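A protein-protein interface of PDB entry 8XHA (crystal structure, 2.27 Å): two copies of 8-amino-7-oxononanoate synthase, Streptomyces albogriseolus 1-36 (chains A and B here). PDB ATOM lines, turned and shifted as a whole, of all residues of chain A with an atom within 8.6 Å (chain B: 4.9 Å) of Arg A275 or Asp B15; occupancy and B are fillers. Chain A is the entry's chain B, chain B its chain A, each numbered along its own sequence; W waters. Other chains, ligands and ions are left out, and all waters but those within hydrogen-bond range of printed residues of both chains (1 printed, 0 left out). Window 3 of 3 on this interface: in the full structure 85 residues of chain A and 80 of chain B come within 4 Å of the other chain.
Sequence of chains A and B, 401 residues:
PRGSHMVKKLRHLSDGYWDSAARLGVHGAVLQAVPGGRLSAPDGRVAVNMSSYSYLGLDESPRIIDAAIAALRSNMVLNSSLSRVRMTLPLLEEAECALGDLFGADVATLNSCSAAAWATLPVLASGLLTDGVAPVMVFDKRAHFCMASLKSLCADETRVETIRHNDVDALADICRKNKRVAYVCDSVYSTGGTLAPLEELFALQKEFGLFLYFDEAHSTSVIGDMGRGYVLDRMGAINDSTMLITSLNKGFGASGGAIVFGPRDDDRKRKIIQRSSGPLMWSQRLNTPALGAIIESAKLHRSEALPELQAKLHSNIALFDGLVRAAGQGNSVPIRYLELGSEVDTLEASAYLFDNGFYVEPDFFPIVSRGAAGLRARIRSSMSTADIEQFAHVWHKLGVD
Water W1 lies within hydrogen-bond range of OD1 of Asp B19 (3.0 Å), NH2 of Arg A275 (3.1 Å) and NZ of Lys A271 (3.5 Å).
Of the printed residues of chain B, Val A85 touches Trp B18 (3.9 Å). Of the printed residues of chain B, Leu A128 touches Arg B11. Arg A270 touches none of the printed residues of chain B. Arg A275 touches four residues of chain B. Of the printed residues of chain A, Arg B11 touches Leu A128 (3.6 Å). No residue of chain A comes within 4 Å of Ser B14. Of the printed residues of chain A, Asp B15 touches Arg A275. No residue of chain A comes within 4 Å of Gly B16. The nearest residue of chain A that does not touch Asp B15 is Ile A272 (6.5 Å). The nearest printed residue of chain B that does not touch Leu A128 is Asp B15 (7.5 Å).
The guanidinium group (NH1) of Arg A275 is in salt-bridge range of the side-chain carboxylate (OD1) of Asp B19, at 3.1 Å.
No position is printed for both chains.
Of the 10 printed residues of chain B, 5 touch a printed residue of chain A. Printed residues of chain B that touch a printed residue of chain A: Arg B11, Asp B15, Trp B18, Asp B19 and Pro B366. Printed residues of chain A that touch a printed residue of chain B: Val A85, Leu A128, Arg A275 and Met A281. Hydrophobic or aromatic side chains of chain A that line the printed part of chain B: Val A85, Leu A128 and Met A281. Among the printed residues, 7 pairs touch across the chains.
Val A85 touches Trp B18 (CG2 to CZ3, 3.9 Å). CD1 of Leu A128 touches NH1 of Arg B11 (3.6 Å). Arg A275 touches Asp B15 (NH1 to O, 3.9 Å). CB of Trp B18 touches NH1 of Arg A275 (3.4 Å). Arg A275 touches Pro B366. Met A281 touches Trp B18.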
ATOM      1  N   VAL A  85       5.985  -7.352  13.863  1.00  0.00           N
ATOM      2  CA  VAL A  85       5.441  -8.374  12.993  1.00  0.00           C
ATOM      3  C   VAL A  85       5.717  -9.768  13.574  1.00  0.00           C
ATOM      4  O   VAL A  85       4.890 -10.683  13.449  1.00  0.00           O
ATOM      5  CB  VAL A  85       6.048  -8.108  11.593  1.00  0.00           C
ATOM      6  CG1 VAL A  85       6.839  -9.265  11.073  1.00  0.00           C
ATOM      7  CG2 VAL A  85       4.984  -7.606  10.618  1.00  0.00           C
ATOM      8  N   ALA A 119       4.046   5.381   6.909  1.00  0.00           N
ATOM      9  CA  ALA A 119       3.517   4.023   6.816  1.00  0.00           C
ATOM     10  C   ALA A 119       2.245   3.942   5.984  1.00  0.00           C
ATOM     11  O   ALA A 119       1.975   2.893   5.387  1.00  0.00           O
ATOM     12  CB  ALA A 119       3.244   3.458   8.213  1.00  0.00           C
ATOM     13  N   VAL A 123       0.874   3.665   0.835  1.00  0.00           N
ATOM     14  CA  VAL A 123      -0.022   2.522   0.701  1.00  0.00           C
ATOM     15  C   VAL A 123      -1.396   2.970   0.212  1.00  0.00           C
ATOM     16  O   VAL A 123      -2.001   2.322  -0.652  1.00  0.00           O
ATOM     17  CB  VAL A 123      -0.100   1.769   2.041  1.00  0.00           C
ATOM     18  CG1 VAL A 123      -1.118   0.638   1.970  1.00  0.00           C
ATOM     19  CG2 VAL A 123       1.286   1.242   2.420  1.00  0.00           C
ATOM     20  N   LEU A 128      -4.220  -0.199  -2.546  1.00  0.00           N
ATOM     21  CA  LEU A 128      -4.469  -1.352  -1.675  1.00  0.00           C
ATOM     22  C   LEU A 128      -5.531  -1.067  -0.626  1.00  0.00           C
ATOM     23  O   LEU A 128      -6.198  -1.991  -0.156  1.00  0.00           O
ATOM     24  CB  LEU A 128      -3.169  -1.788  -0.988  1.00  0.00           C
ATOM     25  CG  LEU A 128      -2.106  -2.372  -1.912  1.00  0.00           C
ATOM     26  CD1 LEU A 128      -0.821  -2.649  -1.150  1.00  0.00           C
ATOM     27  CD2 LEU A 128      -2.639  -3.629  -2.553  1.00  0.00           C
ATOM     28  N   PHE A 261      -7.090   3.305  11.755  1.00  0.00           N
ATOM     29  CA  PHE A 261      -7.279   2.678  10.426  1.00  0.00           C
ATOM     30  C   PHE A 261      -8.712   2.643   9.925  1.00  0.00           C
ATOM     31  O   PHE A 261      -8.890   2.551   8.708  1.00  0.00           O
ATOM     32  CB  PHE A 261      -6.871   1.207  10.504  1.00  0.00           C
ATOM     33  CG  PHE A 261      -5.434   0.904  10.841  1.00  0.00           C
ATOM     34  CD1 PHE A 261      -4.445   0.985   9.877  1.00  0.00           C
ATOM     35  CD2 PHE A 261      -5.082   0.478  12.110  1.00  0.00           C
ATOM     36  CE1 PHE A 261      -3.129   0.684  10.183  1.00  0.00           C
ATOM     37  CE2 PHE A 261      -3.766   0.176  12.415  1.00  0.00           C
ATOM     38  CZ  PHE A 261      -2.792   0.280  11.452  1.00  0.00           C
ATOM     39  N   ASP A 267      -9.997  -5.883  10.111  1.00  0.00           N
ATOM     40  CA  ASP A 267      -8.523  -5.964  10.265  1.00  0.00           C
ATOM     41  C   ASP A 267      -7.826  -5.804   8.919  1.00  0.00           C
ATOM     42  O   ASP A 267      -6.596  -5.857   8.895  1.00  0.00           O
ATOM     43  CB  ASP A 267      -8.137  -7.312  10.869  1.00  0.00           C
ATOM     44  CG  ASP A 267      -8.507  -8.495   9.992  1.00  0.00           C
ATOM     45  OD1 ASP A 267      -9.245  -8.291   9.014  1.00  0.00           O
ATOM     46  OD2 ASP A 267      -8.046  -9.610  10.295  1.00  0.00           O
ATOM     47  N   ARG A 268      -8.585  -5.607   7.852  1.00  0.00           N
ATOM     48  CA  ARG A 268      -7.976  -5.568   6.500  1.00  0.00           C
ATOM     49  C   ARG A 268      -6.956  -4.432   6.390  1.00  0.00           C
ATOM     50  O   ARG A 268      -5.853  -4.687   5.900  1.00  0.00           O
ATOM     51  CB  ARG A 268      -9.090  -5.486   5.455  1.00  0.00           C
ATOM     52  CG  ARG A 268      -9.884  -6.777   5.326  1.00  0.00           C
ATOM     53  CD  ARG A 268     -10.927  -6.783   4.228  1.00  0.00           C
ATOM     54  NE  ARG A 268     -12.150  -6.084   4.594  1.00  0.00           N
ATOM     55  CZ  ARG A 268     -12.463  -4.860   4.198  1.00  0.00           C
ATOM     56  NH1 ARG A 268     -11.642  -4.189   3.410  1.00  0.00           N
ATOM     57  NH2 ARG A 268     -13.600  -4.312   4.585  1.00  0.00           N
ATOM     58  N   LYS A 269      -7.311  -3.234   6.842  1.00  0.00           N
ATOM     59  CA  LYS A 269      -6.399  -2.075   6.688  1.00  0.00           C
ATOM     60  C   LYS A 269      -5.164  -2.279   7.570  1.00  0.00           C
ATOM     61  O   LYS A 269      -4.054  -2.061   7.072  1.00  0.00           O
ATOM     62  CB  LYS A 269      -7.129  -0.764   6.990  1.00  0.00           C
ATOM     63  CG  LYS A 269      -8.124  -0.315   5.931  1.00  0.00           C
ATOM     64  CD  LYS A 269      -8.403   1.169   5.971  1.00  0.00           C
ATOM     65  CE  LYS A 269      -9.376   1.622   4.906  1.00  0.00           C
ATOM     66  NZ  LYS A 269     -10.718   1.027   5.104  1.00  0.00           N
ATOM     67  N   ARG A 270      -5.357  -2.708   8.815  1.00  0.00           N
ATOM     68  CA  ARG A 270      -4.189  -2.984   9.648  1.00  0.00           C
ATOM     69  C   ARG A 270      -3.303  -4.039   8.996  1.00  0.00           C
ATOM     70  O   ARG A 270      -2.089  -3.840   8.842  1.00  0.00           O
ATOM     71  CB  ARG A 270      -4.607  -3.426  11.053  1.00  0.00           C
ATOM     72  CG  ARG A 270      -3.393  -3.800  11.915  1.00  0.00           C
ATOM     73  CD  ARG A 270      -3.750  -4.426  13.258  1.00  0.00           C
ATOM     74  NE  ARG A 270      -4.357  -3.482  14.185  1.00  0.00           N
ATOM     75  CZ  ARG A 270      -3.721  -2.906  15.196  1.00  0.00           C
ATOM     76  NH1 ARG A 270      -2.415  -3.056  15.367  1.00  0.00           N
ATOM     77  NH2 ARG A 270      -4.414  -2.166  16.062  1.00  0.00           N
ATOM     78  N   LYS A 271      -3.905  -5.154   8.577  1.00  0.00           N
ATOM     79  CA  LYS A 271      -3.204  -6.202   7.839  1.00  0.00           C
ATOM     80  C   LYS A 271      -2.381  -5.621   6.695  1.00  0.00           C
ATOM     81  O   LYS A 271      -1.184  -5.895   6.565  1.00  0.00           O
ATOM     82  CB  LYS A 271      -4.228  -7.203   7.282  1.00  0.00           C
ATOM     83  CG  LYS A 271      -4.276  -8.604   7.895  1.00  0.00           C
ATOM     84  CD  LYS A 271      -5.423  -9.403   7.231  1.00  0.00           C
ATOM     85  CE  LYS A 271      -5.520 -10.861   7.687  1.00  0.00           C
ATOM     86  NZ  LYS A 271      -6.217 -11.020   9.011  1.00  0.00           N
ATOM     87  N   ILE A 272      -3.027  -4.812   5.854  1.00  0.00           N
ATOM     88  CA  ILE A 272      -2.389  -4.322   4.634  1.00  0.00           C
ATOM     89  C   ILE A 272      -1.182  -3.456   4.969  1.00  0.00           C
ATOM     90  O   ILE A 272      -0.092  -3.629   4.403  1.00  0.00           O
ATOM     91  CB  ILE A 272      -3.417  -3.560   3.776  1.00  0.00           C
ATOM     92  CG1 ILE A 272      -4.419  -4.542   3.164  1.00  0.00           C
ATOM     93  CG2 ILE A 272      -2.730  -2.715   2.700  1.00  0.00           C
ATOM     94  CD1 ILE A 272      -5.702  -3.882   2.664  1.00  0.00           C
ATOM     95  N   ILE A 273      -1.356  -2.512   5.901  1.00  0.00           N
ATOM     96  CA  ILE A 273      -0.267  -1.607   6.241  1.00  0.00           C
ATOM     97  C   ILE A 273       0.800  -2.338   7.042  1.00  0.00           C
ATOM     98  O   ILE A 273       2.005  -2.172   6.794  1.00  0.00           O
ATOM     99  CB  ILE A 273      -0.820  -0.376   6.983  1.00  0.00           C
ATOM    100  CG1 ILE A 273      -1.628   0.485   6.008  1.00  0.00           C
ATOM    101  CG2 ILE A 273       0.314   0.460   7.600  1.00  0.00           C
ATOM    102  CD1 ILE A 273      -2.880   1.056   6.613  1.00  0.00           C
ATOM    103  N   GLN A 274       0.380  -3.185   7.991  1.00  0.00           N
ATOM    104  CA  GLN A 274       1.348  -3.949   8.778  1.00  0.00           C
ATOM    105  C   GLN A 274       2.219  -4.831   7.893  1.00  0.00           C
ATOM    106  O   GLN A 274       3.390  -5.071   8.214  1.00  0.00           O
ATOM    107  CB  GLN A 274       0.629  -4.798   9.830  1.00  0.00           C
ATOM    108  CG  GLN A 274       1.557  -5.600  10.723  1.00  0.00           C
ATOM    109  CD  GLN A 274       2.476  -4.708  11.551  1.00  0.00           C
ATOM    110  OE1 GLN A 274       2.137  -4.323  12.673  1.00  0.00           O
ATOM    111  NE2 GLN A 274       3.636  -4.366  10.995  1.00  0.00           N
ATOM    112  N   ARG A 275       1.680  -5.296   6.762  1.00  0.00           N
ATOM    113  CA  ARG A 275       2.439  -6.173   5.878  1.00  0.00           C
ATOM    114  C   ARG A 275       3.157  -5.431   4.765  1.00  0.00           C
ATOM    115  O   ARG A 275       3.873  -6.070   3.993  1.00  0.00           O
ATOM    116  CB  ARG A 275       1.516  -7.236   5.280  1.00  0.00           C
ATOM    117  CG  ARG A 275       1.007  -8.157   6.350  1.00  0.00           C
ATOM    118  CD  ARG A 275      -0.100  -9.034   5.867  1.00  0.00           C
ATOM    119  NE  ARG A 275      -0.552  -9.861   6.971  1.00  0.00           N
ATOM    120  CZ  ARG A 275      -1.276 -10.959   6.829  1.00  0.00           C
ATOM    121  NH1 ARG A 275      -1.653 -11.381   5.638  1.00  0.00           N
ATOM    122  NH2 ARG A 275      -1.615 -11.653   7.911  1.00  0.00           N
ATOM    123  N   SER A 276       2.985  -4.110   4.672  1.00  0.00           N
ATOM    124  CA  SER A 276       3.724  -3.261   3.739  1.00  0.00           C
ATOM    125  C   SER A 276       5.086  -2.897   4.307  1.00  0.00           C
ATOM    126  O   SER A 276       5.307  -2.907   5.518  1.00  0.00           O
ATOM    127  CB  SER A 276       2.963  -1.970   3.462  1.00  0.00           C
ATOM    128  OG  SER A 276       1.669  -2.253   2.986  1.00  0.00           O
ATOM    129  N   SER A 277       6.000  -2.514   3.418  1.00  0.00           N
ATOM    130  CA  SER A 277       7.383  -2.300   3.832  1.00  0.00           C
ATOM    131  C   SER A 277       7.572  -0.830   4.199  1.00  0.00           C
ATOM    132  O   SER A 277       8.109  -0.017   3.442  1.00  0.00           O
ATOM    133  CB  SER A 277       8.347  -2.750   2.750  1.00  0.00           C
ATOM    134  OG  SER A 277       9.664  -2.658   3.242  1.00  0.00           O
ATOM    135  N   GLY A 278       7.119  -0.494   5.400  1.00  0.00           N
ATOM    136  CA  GLY A 278       7.242   0.840   5.924  1.00  0.00           C
ATOM    137  C   GLY A 278       7.406   0.825   7.432  1.00  0.00           C
ATOM    138  O   GLY A 278       7.536  -0.236   8.059  1.00  0.00           O
ATOM    139  N   LEU A 280       5.641   0.870  10.052  1.00  0.00           N
ATOM    140  CA  LEU A 280       4.890   0.017  10.963  1.00  0.00           C
ATOM    141  C   LEU A 280       5.478  -1.381  11.022  1.00  0.00           C
ATOM    142  O   LEU A 280       5.388  -2.035  12.072  1.00  0.00           O
ATOM    143  CB  LEU A 280       3.416  -0.048  10.567  1.00  0.00           C
ATOM    144  CG  LEU A 280       2.564  -0.739  11.639  1.00  0.00           C
ATOM    145  CD1 LEU A 280       2.657  -0.003  12.978  1.00  0.00           C
ATOM    146  CD2 LEU A 280       1.147  -0.837  11.186  1.00  0.00           C
ATOM    147  N   MET A 281       6.114  -1.832   9.937  1.00  0.00           N
ATOM    148  CA  MET A 281       6.829  -3.106   9.915  1.00  0.00           C
ATOM    149  C   MET A 281       8.242  -3.012  10.486  1.00  0.00           C
ATOM    150  O   MET A 281       8.615  -3.840  11.326  1.00  0.00           O
ATOM    151  CB  MET A 281       6.909  -3.664   8.486  1.00  0.00           C
ATOM    152  CG  MET A 281       7.806  -4.920   8.390  1.00  0.00           C
ATOM    153  SD  MET A 281       7.907  -5.614   6.703  1.00  0.00           S
ATOM    154  CE  MET A 281       6.201  -6.030   6.394  1.00  0.00           C
ATOM    155  N   TRP A 282       9.048  -2.045  10.038  1.00  0.00           N
ATOM    156  CA  TRP A 282      10.482  -2.066  10.439  1.00  0.00           C
ATOM    157  C   TRP A 282      10.978  -0.866  11.260  1.00  0.00           C
ATOM    158  O   TRP A 282      12.202  -0.726  11.364  1.00  0.00           O
ATOM    159  CB  TRP A 282      11.357  -2.283   9.198  1.00  0.00           C
ATOM    160  CG  TRP A 282      10.962  -1.550   7.954  1.00  0.00           C
ATOM    161  CD1 TRP A 282      10.527  -2.105   6.787  1.00  0.00           C
ATOM    162  CD2 TRP A 282      11.014  -0.131   7.724  1.00  0.00           C
ATOM    163  NE1 TRP A 282      10.289  -1.134   5.856  1.00  0.00           N
ATOM    164  CE2 TRP A 282      10.579   0.087   6.401  1.00  0.00           C
ATOM    165  CE3 TRP A 282      11.373   0.972   8.504  1.00  0.00           C
ATOM    166  CZ2 TRP A 282      10.494   1.362   5.846  1.00  0.00           C
ATOM    167  CZ3 TRP A 282      11.289   2.231   7.955  1.00  0.00           C
ATOM    168  CH2 TRP A 282      10.855   2.421   6.645  1.00  0.00           C
ATOM    169  N   ARG B  11       0.698 -11.296  -5.045  1.00  0.00           N
ATOM    170  CA  ARG B  11       0.113 -10.782  -3.782  1.00  0.00           C
ATOM    171  C   ARG B  11      -0.660 -11.911  -3.103  1.00  0.00           C
ATOM    172  O   ARG B  11      -0.475 -12.090  -1.894  1.00  0.00           O
ATOM    173  CB  ARG B  11      -0.767  -9.558  -4.036  1.00  0.00           C
ATOM    174  CG  ARG B  11       0.014  -8.304  -4.397  1.00  0.00           C
ATOM    175  CD  ARG B  11      -0.862  -7.070  -4.501  1.00  0.00           C
ATOM    176  NE  ARG B  11      -0.133  -5.948  -5.072  1.00  0.00           N
ATOM    177  CZ  ARG B  11       0.638  -5.121  -4.377  1.00  0.00           C
ATOM    178  NH1 ARG B  11       0.787  -5.295  -3.075  1.00  0.00           N
ATOM    179  NH2 ARG B  11       1.261  -4.129  -4.985  1.00  0.00           N
ATOM    180  N   HIS B  12      -1.494 -12.633  -3.848  1.00  0.00           N
ATOM    181  CA  HIS B  12      -2.174 -13.782  -3.254  1.00  0.00           C
ATOM    182  C   HIS B  12      -1.170 -14.780  -2.691  1.00  0.00           C
ATOM    183  O   HIS B  12      -1.422 -15.403  -1.652  1.00  0.00           O
ATOM    184  CB  HIS B  12      -3.085 -14.458  -4.287  1.00  0.00           C
ATOM    185  CG  HIS B  12      -3.884 -15.606  -3.738  1.00  0.00           C
ATOM    186  ND1 HIS B  12      -3.425 -16.907  -3.746  1.00  0.00           N
ATOM    187  CD2 HIS B  12      -5.118 -15.649  -3.175  1.00  0.00           C
ATOM    188  CE1 HIS B  12      -4.336 -17.699  -3.205  1.00  0.00           C
ATOM    189  NE2 HIS B  12      -5.373 -16.962  -2.851  1.00  0.00           N
ATOM    190  N   LEU B  13      -0.024 -14.925  -3.352  1.00  0.00           N
ATOM    191  CA  LEU B  13       1.039 -15.779  -2.839  1.00  0.00           C
ATOM    192  C   LEU B  13       1.603 -15.229  -1.536  1.00  0.00           C
ATOM    193  O   LEU B  13       1.704 -15.953  -0.538  1.00  0.00           O
ATOM    194  CB  LEU B  13       2.143 -15.900  -3.884  1.00  0.00           C
ATOM    195  CG  LEU B  13       3.090 -17.081  -3.771  1.00  0.00           C
ATOM    196  CD1 LEU B  13       2.317 -18.376  -4.001  1.00  0.00           C
ATOM    197  CD2 LEU B  13       4.216 -16.923  -4.780  1.00  0.00           C
ATOM    198  N   SER B  14       1.985 -13.945  -1.538  1.00  0.00           N
ATOM    199  CA  SER B  14       2.563 -13.324  -0.351  1.00  0.00           C
ATOM    200  C   SER B  14       1.577 -13.289   0.802  1.00  0.00           C
ATOM    201  O   SER B  14       1.944 -13.602   1.936  1.00  0.00           O
ATOM    202  CB  SER B  14       3.044 -11.912  -0.669  1.00  0.00           C
ATOM    203  OG  SER B  14       4.373 -11.950  -1.143  1.00  0.00           O
ATOM    204  N   ASP B  15       0.332 -12.893   0.539  1.00  0.00           N
ATOM    205  CA  ASP B  15      -0.686 -12.933   1.583  1.00  0.00           C
ATOM    206  C   ASP B  15      -0.843 -14.331   2.150  1.00  0.00           C
ATOM    207  O   ASP B  15      -1.195 -14.481   3.322  1.00  0.00           O
ATOM    208  CB  ASP B  15      -2.037 -12.449   1.055  1.00  0.00           C
ATOM    209  CG  ASP B  15      -2.062 -10.961   0.780  1.00  0.00           C
ATOM    210  OD1 ASP B  15      -0.987 -10.327   0.751  1.00  0.00           O
ATOM    211  OD2 ASP B  15      -3.168 -10.422   0.587  1.00  0.00           O
ATOM    212  N   GLY B  16      -0.606 -15.361   1.337  1.00  0.00           N
ATOM    213  CA  GLY B  16      -0.668 -16.720   1.848  1.00  0.00           C
ATOM    214  C   GLY B  16       0.449 -17.024   2.830  1.00  0.00           C
ATOM    215  O   GLY B  16       0.233 -17.691   3.842  1.00  0.00           O
ATOM    216  N   TYR B  17       1.659 -16.530   2.552  1.00  0.00           N
ATOM    217  CA  TYR B  17       2.778 -16.774   3.455  1.00  0.00           C
ATOM    218  C   TYR B  17       2.596 -16.032   4.783  1.00  0.00           C
ATOM    219  O   TYR B  17       2.898 -16.572   5.855  1.00  0.00           O
ATOM    220  CB  TYR B  17       4.096 -16.372   2.787  1.00  0.00           C
ATOM    221  CG  TYR B  17       4.468 -17.179   1.550  1.00  0.00           C
ATOM    222  CD1 TYR B  17       4.131 -18.527   1.425  1.00  0.00           C
ATOM    223  CD2 TYR B  17       5.153 -16.580   0.506  1.00  0.00           C
ATOM    224  CE1 TYR B  17       4.475 -19.249   0.282  1.00  0.00           C
ATOM    225  CE2 TYR B  17       5.493 -17.282  -0.624  1.00  0.00           C
ATOM    226  CZ  TYR B  17       5.158 -18.605  -0.734  1.00  0.00           C
ATOM    227  OH  TYR B  17       5.524 -19.263  -1.876  1.00  0.00           O
ATOM    228  N   TRP B  18       2.124 -14.778   4.731  1.00  0.00           N
ATOM    229  CA  TRP B  18       1.887 -14.032   5.966  1.00  0.00           C
ATOM    230  C   TRP B  18       0.770 -14.662   6.774  1.00  0.00           C
ATOM    231  O   TRP B  18       0.810 -14.661   8.009  1.00  0.00           O
ATOM    232  CB  TRP B  18       1.547 -12.572   5.663  1.00  0.00           C
ATOM    233  CG  TRP B  18       2.700 -11.800   5.184  1.00  0.00           C
ATOM    234  CD1 TRP B  18       3.057 -11.590   3.889  1.00  0.00           C
ATOM    235  CD2 TRP B  18       3.673 -11.130   5.987  1.00  0.00           C
ATOM    236  NE1 TRP B  18       4.201 -10.831   3.835  1.00  0.00           N
ATOM    237  CE2 TRP B  18       4.592 -10.529   5.112  1.00  0.00           C
ATOM    238  CE3 TRP B  18       3.848 -10.968   7.358  1.00  0.00           C
ATOM    239  CZ2 TRP B  18       5.678  -9.781   5.568  1.00  0.00           C
ATOM    240  CZ3 TRP B  18       4.920 -10.235   7.804  1.00  0.00           C
ATOM    241  CH2 TRP B  18       5.820  -9.649   6.921  1.00  0.00           C
ATOM    242  N   ASP B  19      -0.253 -15.188   6.094  1.00  0.00           N
ATOM    243  CA  ASP B  19      -1.334 -15.863   6.810  1.00  0.00           C
ATOM    244  C   ASP B  19      -0.840 -17.139   7.476  1.00  0.00           C
ATOM    245  O   ASP B  19      -1.229 -17.441   8.608  1.00  0.00           O
ATOM    246  CB  ASP B  19      -2.492 -16.165   5.860  1.00  0.00           C
ATOM    247  CG  ASP B  19      -3.282 -14.923   5.492  1.00  0.00           C
ATOM    248  OD1 ASP B  19      -3.245 -13.929   6.255  1.00  0.00           O
ATOM    249  OD2 ASP B  19      -3.950 -14.945   4.440  1.00  0.00           O
ATOM    250  N   PRO B 366       7.793  -9.841   1.538  1.00  0.00           N
ATOM    251  CA  PRO B 366       8.708  -8.790   1.055  1.00  0.00           C
ATOM    252  C   PRO B 366       9.948  -8.471   1.877  1.00  0.00           C
ATOM    253  O   PRO B 366      10.627  -7.505   1.526  1.00  0.00           O
ATOM    254  CB  PRO B 366       7.812  -7.549   1.044  1.00  0.00           C
ATOM    255  CG  PRO B 366       6.844  -7.795   2.163  1.00  0.00           C
ATOM    256  CD  PRO B 366       6.543  -9.270   2.082  1.00  0.00           C
HETATM  257  O   HOH W   1      -3.782 -13.512   9.226  1.00  0.00           O
